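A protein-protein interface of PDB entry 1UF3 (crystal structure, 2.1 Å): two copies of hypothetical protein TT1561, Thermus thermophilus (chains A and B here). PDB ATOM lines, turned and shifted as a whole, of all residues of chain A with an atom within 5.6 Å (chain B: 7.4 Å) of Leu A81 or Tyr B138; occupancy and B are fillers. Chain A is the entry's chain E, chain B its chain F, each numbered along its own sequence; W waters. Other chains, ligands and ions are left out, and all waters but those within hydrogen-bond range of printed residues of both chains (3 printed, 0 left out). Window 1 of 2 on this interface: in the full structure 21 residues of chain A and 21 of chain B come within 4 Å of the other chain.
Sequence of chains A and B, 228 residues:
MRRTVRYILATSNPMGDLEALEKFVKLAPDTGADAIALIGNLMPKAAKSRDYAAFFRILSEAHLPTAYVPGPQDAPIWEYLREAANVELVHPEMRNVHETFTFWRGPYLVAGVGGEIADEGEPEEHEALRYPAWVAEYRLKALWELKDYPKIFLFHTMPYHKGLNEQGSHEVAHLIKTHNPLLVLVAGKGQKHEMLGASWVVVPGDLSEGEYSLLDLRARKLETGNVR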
ATOM      1  N   ILE A  77      26.642 -26.197  21.568  1.00  0.00           N
ATOM      2  CA  ILE A  77      25.413 -25.401  21.618  1.00  0.00           C
ATOM      3  C   ILE A  77      24.546 -25.438  20.369  1.00  0.00           C
ATOM      4  O   ILE A  77      23.314 -25.512  20.454  1.00  0.00           O
ATOM      5  CB  ILE A  77      25.749 -23.903  21.988  1.00  0.00           C
ATOM      6  CG1 ILE A  77      24.467 -23.101  22.209  1.00  0.00           C
ATOM      7  CG2 ILE A  77      26.572 -23.241  20.869  1.00  0.00           C
ATOM      8  CD1 ILE A  77      23.623 -23.557  23.404  1.00  0.00           C
ATOM      9  N   TRP A  78      25.179 -25.419  19.202  1.00  0.00           N
ATOM     10  CA  TRP A  78      24.421 -25.382  17.956  1.00  0.00           C
ATOM     11  C   TRP A  78      23.555 -26.606  17.654  1.00  0.00           C
ATOM     12  O   TRP A  78      22.565 -26.493  16.928  1.00  0.00           O
ATOM     13  CB  TRP A  78      25.357 -25.058  16.779  1.00  0.00           C
ATOM     14  CG  TRP A  78      26.263 -23.866  17.041  1.00  0.00           C
ATOM     15  CD1 TRP A  78      27.610 -23.900  17.287  1.00  0.00           C
ATOM     16  CD2 TRP A  78      25.879 -22.477  17.122  1.00  0.00           C
ATOM     17  NE1 TRP A  78      28.080 -22.630  17.518  1.00  0.00           N
ATOM     18  CE2 TRP A  78      27.043 -21.740  17.422  1.00  0.00           C
ATOM     19  CE3 TRP A  78      24.663 -21.788  16.972  1.00  0.00           C
ATOM     20  CZ2 TRP A  78      27.031 -20.335  17.576  1.00  0.00           C
ATOM     21  CZ3 TRP A  78      24.655 -20.397  17.132  1.00  0.00           C
ATOM     22  CH2 TRP A  78      25.829 -19.692  17.429  1.00  0.00           C
ATOM     23  N   GLU A  79      23.875 -27.771  18.213  1.00  0.00           N
ATOM     24  CA  GLU A  79      23.024 -28.921  17.937  1.00  0.00           C
ATOM     25  C   GLU A  79      21.691 -28.760  18.672  1.00  0.00           C
ATOM     26  O   GLU A  79      20.623 -29.012  18.115  1.00  0.00           O
ATOM     27  CB  GLU A  79      23.736 -30.218  18.325  1.00  0.00           C
ATOM     28  CG  GLU A  79      24.951 -30.480  17.450  1.00  0.00           C
ATOM     29  CD  GLU A  79      25.586 -31.842  17.692  1.00  0.00           C
ATOM     30  OE1 GLU A  79      26.558 -32.170  16.973  1.00  0.00           O
ATOM     31  OE2 GLU A  79      25.116 -32.576  18.591  1.00  0.00           O
ATOM     32  N   TYR A  80      21.762 -28.344  19.933  1.00  0.00           N
ATOM     33  CA  TYR A  80      20.568 -28.072  20.732  1.00  0.00           C
ATOM     34  C   TYR A  80      19.839 -26.906  20.046  1.00  0.00           C
ATOM     35  O   TYR A  80      18.631 -26.972  19.783  1.00  0.00           O
ATOM     36  CB  TYR A  80      20.989 -27.658  22.146  1.00  0.00           C
ATOM     37  CG  TYR A  80      19.944 -26.893  22.949  1.00  0.00           C
ATOM     38  CD1 TYR A  80      18.916 -27.558  23.615  1.00  0.00           C
ATOM     39  CD2 TYR A  80      20.004 -25.495  23.050  1.00  0.00           C
ATOM     40  CE1 TYR A  80      17.976 -26.858  24.362  1.00  0.00           C
ATOM     41  CE2 TYR A  80      19.066 -24.784  23.800  1.00  0.00           C
ATOM     42  CZ  TYR A  80      18.057 -25.476  24.455  1.00  0.00           C
ATOM     43  OH  TYR A  80      17.146 -24.783  25.212  1.00  0.00           O
ATOM     44  N   LEU A  81      20.574 -25.842  19.733  1.00  0.00           N
ATOM     45  CA  LEU A  81      19.941 -24.675  19.101  1.00  0.00           C
ATOM     46  C   LEU A  81      19.248 -25.019  17.787  1.00  0.00           C
ATOM     47  O   LEU A  81      18.140 -24.544  17.522  1.00  0.00           O
ATOM     48  CB  LEU A  81      20.968 -23.561  18.862  1.00  0.00           C
ATOM     49  CG  LEU A  81      20.386 -22.174  18.558  1.00  0.00           C
ATOM     50  CD1 LEU A  81      19.639 -21.656  19.818  1.00  0.00           C
ATOM     51  CD2 LEU A  81      21.496 -21.201  18.193  1.00  0.00           C
ATOM     52  N   ARG A  82      19.881 -25.864  16.967  1.00  0.00           N
ATOM     53  CA  ARG A  82      19.286 -26.222  15.685  1.00  0.00           C
ATOM     54  C   ARG A  82      18.022 -27.066  15.811  1.00  0.00           C
ATOM     55  O   ARG A  82      17.020 -26.806  15.127  1.00  0.00           O
ATOM     56  CB  ARG A  82      20.290 -26.949  14.788  1.00  0.00           C
ATOM     57  CG  ARG A  82      19.736 -27.191  13.401  1.00  0.00           C
ATOM     58  CD  ARG A  82      19.174 -25.903  12.858  1.00  0.00           C
ATOM     59  NE  ARG A  82      18.423 -26.053  11.616  1.00  0.00           N
ATOM     60  CZ  ARG A  82      18.958 -26.389  10.448  1.00  0.00           C
ATOM     61  NH1 ARG A  82      20.264 -26.626  10.350  1.00  0.00           N
ATOM     62  NH2 ARG A  82      18.186 -26.458   9.370  1.00  0.00           N
ATOM     63  N   GLU A  83      18.049 -28.072  16.681  1.00  0.00           N
ATOM     64  CA  GLU A  83      16.864 -28.883  16.836  1.00  0.00           C
ATOM     65  C   GLU A  83      15.789 -28.087  17.541  1.00  0.00           C
ATOM     66  O   GLU A  83      14.612 -28.307  17.291  1.00  0.00           O
ATOM     67  CB  GLU A  83      17.174 -30.173  17.593  1.00  0.00           C
ATOM     68  CG  GLU A  83      18.102 -31.094  16.813  1.00  0.00           C
ATOM     69  CD  GLU A  83      17.593 -31.391  15.410  1.00  0.00           C
ATOM     70  OE1 GLU A  83      18.445 -31.643  14.529  1.00  0.00           O
ATOM     71  OE2 GLU A  83      16.360 -31.376  15.184  1.00  0.00           O
ATOM     72  N   ALA A  84      16.171 -27.171  18.429  1.00  0.00           N
ATOM     73  CA  ALA A  84      15.160 -26.335  19.091  1.00  0.00           C
ATOM     74  C   ALA A  84      14.513 -25.493  17.966  1.00  0.00           C
ATOM     75  O   ALA A  84      13.303 -25.476  17.809  1.00  0.00           O
ATOM     76  CB  ALA A  84      15.813 -25.411  20.126  1.00  0.00           C
ATOM     77  N   ALA A  85      15.337 -24.818  17.171  1.00  0.00           N
ATOM     78  CA  ALA A  85      14.819 -23.999  16.071  1.00  0.00           C
ATOM     79  C   ALA A  85      13.868 -24.797  15.166  1.00  0.00           C
ATOM     80  O   ALA A  85      12.759 -24.335  14.843  1.00  0.00           O
ATOM     81  CB  ALA A  85      15.983 -23.433  15.246  1.00  0.00           C
ATOM     82  N   ASN A  86      14.294 -25.998  14.770  1.00  0.00           N
ATOM     83  CA  ASN A  86      13.476 -26.847  13.903  1.00  0.00           C
ATOM     84  C   ASN A  86      12.092 -27.203  14.449  1.00  0.00           C
ATOM     85  O   ASN A  86      11.108 -27.153  13.707  1.00  0.00           O
ATOM     86  CB  ASN A  86      14.192 -28.166  13.558  1.00  0.00           C
ATOM     87  CG  ASN A  86      15.346 -27.978  12.566  1.00  0.00           C
ATOM     88  OD1 ASN A  86      15.391 -26.993  11.820  1.00  0.00           O
ATOM     89  ND2 ASN A  86      16.277 -28.941  12.549  1.00  0.00           N
ATOM     90  N   GLU A  88      10.491 -25.641  16.936  1.00  0.00           N
ATOM     91  CA  GLU A  88       9.728 -24.418  17.217  1.00  0.00           C
ATOM     92  C   GLU A  88       9.073 -23.769  15.998  1.00  0.00           C
ATOM     93  O   GLU A  88       8.081 -23.037  16.131  1.00  0.00           O
ATOM     94  CB  GLU A  88      10.598 -23.418  17.966  1.00  0.00           C
ATOM     95  CG  GLU A  88      10.811 -23.817  19.421  1.00  0.00           C
ATOM     96  CD  GLU A  88      12.022 -23.179  20.038  1.00  0.00           C
ATOM     97  OE1 GLU A  88      12.327 -22.020  19.686  1.00  0.00           O
ATOM     98  OE2 GLU A  88      12.664 -23.824  20.899  1.00  0.00           O
ATOM     99  N   ARG A  95       9.411 -23.098  23.287  1.00  0.00           N
ATOM    100  CA  ARG A  95      10.398 -22.054  23.240  1.00  0.00           C
ATOM    101  C   ARG A  95      11.624 -22.207  24.106  1.00  0.00           C
ATOM    102  O   ARG A  95      11.543 -22.278  25.322  1.00  0.00           O
ATOM    103  CB  ARG A  95       9.740 -20.718  23.557  1.00  0.00           C
ATOM    104  CG  ARG A  95      10.652 -19.518  23.441  1.00  0.00           C
ATOM    105  CD  ARG A  95      11.356 -19.421  22.041  1.00  0.00           C
ATOM    106  NE  ARG A  95      11.600 -18.034  21.660  1.00  0.00           N
ATOM    107  CZ  ARG A  95      12.720 -17.566  21.113  1.00  0.00           C
ATOM    108  NH1 ARG A  95      13.752 -18.368  20.867  1.00  0.00           N
ATOM    109  NH2 ARG A  95      12.799 -16.275  20.809  1.00  0.00           N
ATOM    110  N   ASN A  96      12.769 -22.273  23.444  1.00  0.00           N
ATOM    111  CA  ASN A  96      14.046 -22.324  24.118  1.00  0.00           C
ATOM    112  C   ASN A  96      14.221 -20.847  24.557  1.00  0.00           C
ATOM    113  O   ASN A  96      14.137 -19.937  23.707  1.00  0.00           O
ATOM    114  CB  ASN A  96      15.107 -22.736  23.097  1.00  0.00           C
ATOM    115  CG  ASN A  96      16.451 -22.144  23.390  1.00  0.00           C
ATOM    116  OD1 ASN A  96      16.945 -22.249  24.496  1.00  0.00           O
ATOM    117  ND2 ASN A  96      17.055 -21.498  22.388  1.00  0.00           N
ATOM    118  N   THR A 100      17.271 -15.511  25.824  1.00  0.00           N
ATOM    119  CA  THR A 100      16.174 -14.779  25.192  1.00  0.00           C
ATOM    120  C   THR A 100      14.903 -14.761  26.081  1.00  0.00           C
ATOM    121  O   THR A 100      14.993 -14.957  27.304  1.00  0.00           O
ATOM    122  CB  THR A 100      15.922 -15.324  23.726  1.00  0.00           C
ATOM    123  OG1 THR A 100      14.986 -14.484  23.043  1.00  0.00           O
ATOM    124  CG2 THR A 100      15.421 -16.753  23.733  1.00  0.00           C
ATOM    125  N   GLU B  99      21.990  -9.996  18.123  1.00  0.00           N
ATOM    126  CA  GLU B  99      21.129 -11.043  18.665  1.00  0.00           C
ATOM    127  C   GLU B  99      20.116 -10.571  19.717  1.00  0.00           C
ATOM    128  O   GLU B  99      19.406 -11.389  20.288  1.00  0.00           O
ATOM    129  CB  GLU B  99      21.961 -12.168  19.273  1.00  0.00           C
ATOM    130  CG  GLU B  99      23.074 -12.654  18.372  1.00  0.00           C
ATOM    131  CD  GLU B  99      23.839 -13.794  19.010  1.00  0.00           C
ATOM    132  OE1 GLU B  99      23.757 -13.946  20.251  1.00  0.00           O
ATOM    133  OE2 GLU B  99      24.526 -14.517  18.269  1.00  0.00           O
ATOM    134  N   VAL B 113      21.764  -8.386  13.647  1.00  0.00           N
ATOM    135  CA  VAL B 113      22.489  -9.642  13.596  1.00  0.00           C
ATOM    136  C   VAL B 113      23.752  -9.278  12.801  1.00  0.00           C
ATOM    137  O   VAL B 113      23.704  -9.055  11.575  1.00  0.00           O
ATOM    138  CB  VAL B 113      21.741 -10.795  12.873  1.00  0.00           C
ATOM    139  CG1 VAL B 113      22.629 -12.043  12.893  1.00  0.00           C
ATOM    140  CG2 VAL B 113      20.403 -11.126  13.560  1.00  0.00           C
ATOM    141  N   PRO B 123      28.004 -22.571  12.140  1.00  0.00           N
ATOM    142  CA  PRO B 123      28.228 -21.270  12.769  1.00  0.00           C
ATOM    143  C   PRO B 123      29.678 -21.248  13.196  1.00  0.00           C
ATOM    144  O   PRO B 123      30.250 -22.302  13.464  1.00  0.00           O
ATOM    145  CB  PRO B 123      27.295 -21.292  13.993  1.00  0.00           C
ATOM    146  CG  PRO B 123      26.285 -22.380  13.681  1.00  0.00           C
ATOM    147  CD  PRO B 123      27.130 -23.415  12.972  1.00  0.00           C
ATOM    148  N   PRO B 132      24.826 -19.127   9.845  1.00  0.00           N
ATOM    149  CA  PRO B 132      24.012 -19.473   8.684  1.00  0.00           C
ATOM    150  C   PRO B 132      22.648 -18.821   8.863  1.00  0.00           C
ATOM    151  O   PRO B 132      22.297 -18.433   9.979  1.00  0.00           O
ATOM    152  CB  PRO B 132      23.956 -20.994   8.745  1.00  0.00           C
ATOM    153  CG  PRO B 132      24.019 -21.281  10.198  1.00  0.00           C
ATOM    154  CD  PRO B 132      25.059 -20.298  10.707  1.00  0.00           C
ATOM    155  N   ALA B 133      21.883 -18.706   7.781  1.00  0.00           N
ATOM    156  CA  ALA B 133      20.572 -18.076   7.831  1.00  0.00           C
ATOM    157  C   ALA B 133      19.621 -18.557   8.942  1.00  0.00           C
ATOM    158  O   ALA B 133      18.999 -17.731   9.601  1.00  0.00           O
ATOM    159  CB  ALA B 133      19.875 -18.205   6.468  1.00  0.00           C
ATOM    160  N   TRP B 134      19.500 -19.864   9.162  1.00  0.00           N
ATOM    161  CA  TRP B 134      18.571 -20.318  10.203  1.00  0.00           C
ATOM    162  C   TRP B 134      18.851 -19.686  11.554  1.00  0.00           C
ATOM    163  O   TRP B 134      17.931 -19.476  12.342  1.00  0.00           O
ATOM    164  CB  TRP B 134      18.540 -21.854  10.325  1.00  0.00           C
ATOM    165  CG  TRP B 134      19.779 -22.480  10.868  1.00  0.00           C
ATOM    166  CD1 TRP B 134      20.809 -22.995  10.152  1.00  0.00           C
ATOM    167  CD2 TRP B 134      20.108 -22.670  12.247  1.00  0.00           C
ATOM    168  NE1 TRP B 134      21.770 -23.499  10.995  1.00  0.00           N
ATOM    169  CE2 TRP B 134      21.365 -23.314  12.290  1.00  0.00           C
ATOM    170  CE3 TRP B 134      19.464 -22.364  13.453  1.00  0.00           C
ATOM    171  CZ2 TRP B 134      21.999 -23.661  13.503  1.00  0.00           C
ATOM    172  CZ3 TRP B 134      20.096 -22.712  14.668  1.00  0.00           C
ATOM    173  CH2 TRP B 134      21.350 -23.353  14.673  1.00  0.00           C
ATOM    174  N   VAL B 135      20.103 -19.337  11.822  1.00  0.00           N
ATOM    175  CA  VAL B 135      20.406 -18.706  13.095  1.00  0.00           C
ATOM    176  C   VAL B 135      19.970 -17.237  13.117  1.00  0.00           C
ATOM    177  O   VAL B 135      19.474 -16.746  14.140  1.00  0.00           O
ATOM    178  CB  VAL B 135      21.912 -18.779  13.445  1.00  0.00           C
ATOM    179  CG1 VAL B 135      22.228 -17.886  14.674  1.00  0.00           C
ATOM    180  CG2 VAL B 135      22.304 -20.243  13.727  1.00  0.00           C
ATOM    181  N   ALA B 136      20.141 -16.522  12.004  1.00  0.00           N
ATOM    182  CA  ALA B 136      19.737 -15.111  12.006  1.00  0.00           C
ATOM    183  C   ALA B 136      18.209 -15.059  12.113  1.00  0.00           C
ATOM    184  O   ALA B 136      17.667 -14.222  12.823  1.00  0.00           O
ATOM    185  CB  ALA B 136      20.245 -14.367  10.728  1.00  0.00           C
ATOM    186  N   GLU B 137      17.524 -15.962  11.426  1.00  0.00           N
ATOM    187  CA  GLU B 137      16.074 -15.999  11.504  1.00  0.00           C
ATOM    188  C   GLU B 137      15.599 -16.308  12.937  1.00  0.00           C
ATOM    189  O   GLU B 137      14.605 -15.752  13.415  1.00  0.00           O
ATOM    190  CB  GLU B 137      15.511 -17.041  10.548  1.00  0.00           C
ATOM    191  CG  GLU B 137      14.003 -16.992  10.505  1.00  0.00           C
ATOM    192  CD  GLU B 137      13.439 -17.661   9.288  1.00  0.00           C
ATOM    193  OE1 GLU B 137      13.336 -18.911   9.278  1.00  0.00           O
ATOM    194  OE2 GLU B 137      13.103 -16.926   8.335  1.00  0.00           O
ATOM    195  N   TYR B 138      16.332 -17.175  13.627  1.00  0.00           N
ATOM    196  CA  TYR B 138      15.984 -17.542  14.994  1.00  0.00           C
ATOM    197  C   TYR B 138      16.137 -16.351  15.944  1.00  0.00           C
ATOM    198  O   TYR B 138      15.326 -16.155  16.849  1.00  0.00           O
ATOM    199  CB  TYR B 138      16.859 -18.714  15.484  1.00  0.00           C
ATOM    200  CG  TYR B 138      16.339 -19.372  16.751  1.00  0.00           C
ATOM    201  CD1 TYR B 138      15.275 -20.270  16.709  1.00  0.00           C
ATOM    202  CD2 TYR B 138      16.905 -19.077  17.993  1.00  0.00           C
ATOM    203  CE1 TYR B 138      14.783 -20.862  17.862  1.00  0.00           C
ATOM    204  CE2 TYR B 138      16.422 -19.661  19.161  1.00  0.00           C
ATOM    205  CZ  TYR B 138      15.358 -20.550  19.088  1.00  0.00           C
ATOM    206  OH  TYR B 138      14.844 -21.091  20.246  1.00  0.00           O
ATOM    207  N   ARG B 139      17.169 -15.541  15.744  1.00  0.00           N
ATOM    208  CA  ARG B 139      17.369 -14.403  16.627  1.00  0.00           C
ATOM    209  C   ARG B 139      16.239 -13.406  16.498  1.00  0.00           C
ATOM    210  O   ARG B 139      15.726 -12.904  17.507  1.00  0.00           O
ATOM    211  CB  ARG B 139      18.680 -13.672  16.320  1.00  0.00           C
ATOM    212  CG  ARG B 139      19.946 -14.536  16.303  1.00  0.00           C
ATOM    213  CD  ARG B 139      20.161 -15.249  17.615  1.00  0.00           C
ATOM    214  NE  ARG B 139      21.468 -15.906  17.669  1.00  0.00           N
ATOM    215  CZ  ARG B 139      21.784 -16.842  18.558  1.00  0.00           C
ATOM    216  NH1 ARG B 139      20.874 -17.233  19.451  1.00  0.00           N
ATOM    217  NH2 ARG B 139      23.012 -17.356  18.588  1.00  0.00           N
ATOM    218  N   LEU B 140      15.867 -13.106  15.254  1.00  0.00           N
ATOM    219  CA  LEU B 140      14.832 -12.112  14.984  1.00  0.00           C
ATOM    220  C   LEU B 140      13.404 -12.551  15.302  1.00  0.00           C
ATOM    221  O   LEU B 140      12.540 -11.706  15.527  1.00  0.00           O
ATOM    222  CB  LEU B 140      14.939 -11.604  13.524  1.00  0.00           C
ATOM    223  CG  LEU B 140      16.262 -10.859  13.229  1.00  0.00           C
ATOM    224  CD1 LEU B 140      16.403 -10.524  11.771  1.00  0.00           C
ATOM    225  CD2 LEU B 140      16.352  -9.577  14.070  1.00  0.00           C
ATOM    226  N   LYS B 141      13.145 -13.851  15.342  1.00  0.00           N
ATOM    227  CA  LYS B 141      11.787 -14.308  15.640  1.00  0.00           C
ATOM    228  C   LYS B 141      11.335 -13.838  17.027  1.00  0.00           C
ATOM    229  O   LYS B 141      10.144 -13.755  17.302  1.00  0.00           O
ATOM    230  CB  LYS B 141      11.661 -15.834  15.526  1.00  0.00           C
ATOM    231  CG  LYS B 141      12.083 -16.607  16.765  1.00  0.00           C
ATOM    232  CD  LYS B 141      11.701 -18.065  16.595  1.00  0.00           C
ATOM    233  CE  LYS B 141      11.913 -18.868  17.876  1.00  0.00           C
ATOM    234  NZ  LYS B 141      11.444 -20.269  17.683  1.00  0.00           N
ATOM    235  N   ALA B 142      12.285 -13.496  17.881  1.00  0.00           N
ATOM    236  CA  ALA B 142      11.958 -13.009  19.213  1.00  0.00           C
ATOM    237  C   ALA B 142      11.237 -11.656  19.109  1.00  0.00           C
ATOM    238  O   ALA B 142      10.495 -11.273  20.028  1.00  0.00           O
ATOM    239  CB  ALA B 142      13.231 -12.856  20.042  1.00  0.00           C
ATOM    240  N   LEU B 143      11.442 -10.932  17.998  1.00  0.00           N
ATOM    241  CA  LEU B 143      10.789  -9.635  17.852  1.00  0.00           C
ATOM    242  C   LEU B 143       9.271  -9.749  17.674  1.00  0.00           C
ATOM    243  O   LEU B 143       8.544  -8.765  17.821  1.00  0.00           O
ATOM    244  CB  LEU B 143      11.424  -8.834  16.704  1.00  0.00           C
ATOM    245  CG  LEU B 143      12.964  -8.704  16.839  1.00  0.00           C
ATOM    246  CD1 LEU B 143      13.508  -7.979  15.617  1.00  0.00           C
ATOM    247  CD2 LEU B 143      13.346  -7.937  18.090  1.00  0.00           C
ATOM    248  N   LEU B 175      14.365 -11.862   5.601  1.00  0.00           N
ATOM    249  CA  LEU B 175      14.172 -11.376   6.973  1.00  0.00           C
ATOM    250  C   LEU B 175      13.564  -9.968   6.951  1.00  0.00           C
ATOM    251  O   LEU B 175      12.738  -9.614   7.805  1.00  0.00           O
ATOM    252  CB  LEU B 175      15.508 -11.313   7.724  1.00  0.00           C
ATOM    253  CG  LEU B 175      16.275 -12.619   7.985  1.00  0.00           C
ATOM    254  CD1 LEU B 175      17.640 -12.280   8.583  1.00  0.00           C
ATOM    255  CD2 LEU B 175      15.484 -13.528   8.910  1.00  0.00           C
HETATM  256  O   HOH W   1       8.739 -20.083  16.948  1.00  0.00           O
HETATM  257  O   HOH W   2      15.694 -16.440  19.761  1.00  0.00           O
HETATM  258  O   HOH W   3      12.290 -21.558  15.249  1.00  0.00           O
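OH of Tyr B138 is in hydrogen-bond range of OE1 of Glu A88, 2.7 Å away.
The side-chain amino group (NZ) of Lys B141 lies within salt-bridge range of the side-chain carboxylate (OE1) of Glu A88 (2.8 Å).
The side-chain hydroxyl of Tyr B138 lies within hydrogen-bond range of the guanidinium group of Arg A95, at 3.0 Å.
The side-chain amide nitrogen (ND2) of Asn A96 is in hydrogen-bond range of the side-chain hydroxyl (OH) of Tyr B138, at 3.1 Å.
OD1 of Asn A96 sits at hydrogen-bond distance from OH of Tyr A80 (2.6 Å).
The guanidinium group (NE) of Arg A82 lies within hydrogen-bond range of the side-chain amide oxygen (OD1) of Asn A86 (3.2 Å).
OE2 of Glu A88 lies within hydrogen-bond range of N of Asn A96 (3.0 Å).
The side-chain carboxylate (OE2) of Glu B99 lies within salt-bridge range of the guanidinium group (NH2) of Arg B139 (3.2 Å).
CG of Pro B123 touches CD2 of Trp A78, at 3.5 Å.
Trp A78 touches Arg B139 (CZ3 to NH2, 3.8 Å).
Leu A81 touches Trp B134.
Leu A81 touches Tyr B138.
Arg A82 touches Trp B134 (CD to CD2, 3.4 Å).
Tyr B138 touches Ala A85 (CD1 to CB, 3.6 Å).
NH1 of Arg A95 touches CE of Lys B141, 3.5 Å away.
NH2 of Arg A95 touches CB of Ala B142 (3.5 Å).
Thr A100 touches Ala B142 (OG1 to CB, 3.8 Å).
Of chain B, only Trp B134 (3.9 Å) and Tyr B138 (3.8 Å) come within 4 Å of Leu A81.
Printed residues of chain B within 4 Å of Arg A82: Trp B134.
Of the printed residues of chain B, Ala A85 touches Tyr B138 (3.6 Å).
Of the printed residues of chain B, Arg A95 touches Tyr B138 (3.0 Å), Lys B141 (3.5 Å) and Ala B142 (3.5 Å).
Printed residues of chain A within 4 Å of Pro B123: Trp A78 (3.5 Å).
Tyr B138 touches just these residues of chain A: Leu A81, Ala A85, Glu A88, Arg A95 and Asn A96.
Of the printed residues of chain A, Arg B139 touches Trp A78.
The nearest residue of chain A that does not touch Tyr B138 is Ala A84 (4.4 Å).
Among the printed residues, Asp or Glu carboxylates within 4 Å of a Lys or Arg side-chain nitrogen of the other chain: Glu A88 with Lys B141.
No position is printed for both chains.
Of the 13 pairs that touch across the chains among the printed residues, none has its exchanged pair printed and touching as well.
Water W1 bridges the side-chain amino group of Lys B141 (2.8 Å) and the backbone carbonyl oxygen of Glu A88 (3.1 Å).
Water W3 bridges the backbone carbonyl oxygen of Ala A85 and the side-chain amino group of Lys B141.
Water W2 lies within hydrogen-bond range of the backbone carbonyl oxygen of Tyr B138 (2.9 Å) and the guanidinium group of Arg A95 (3.0 Å).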
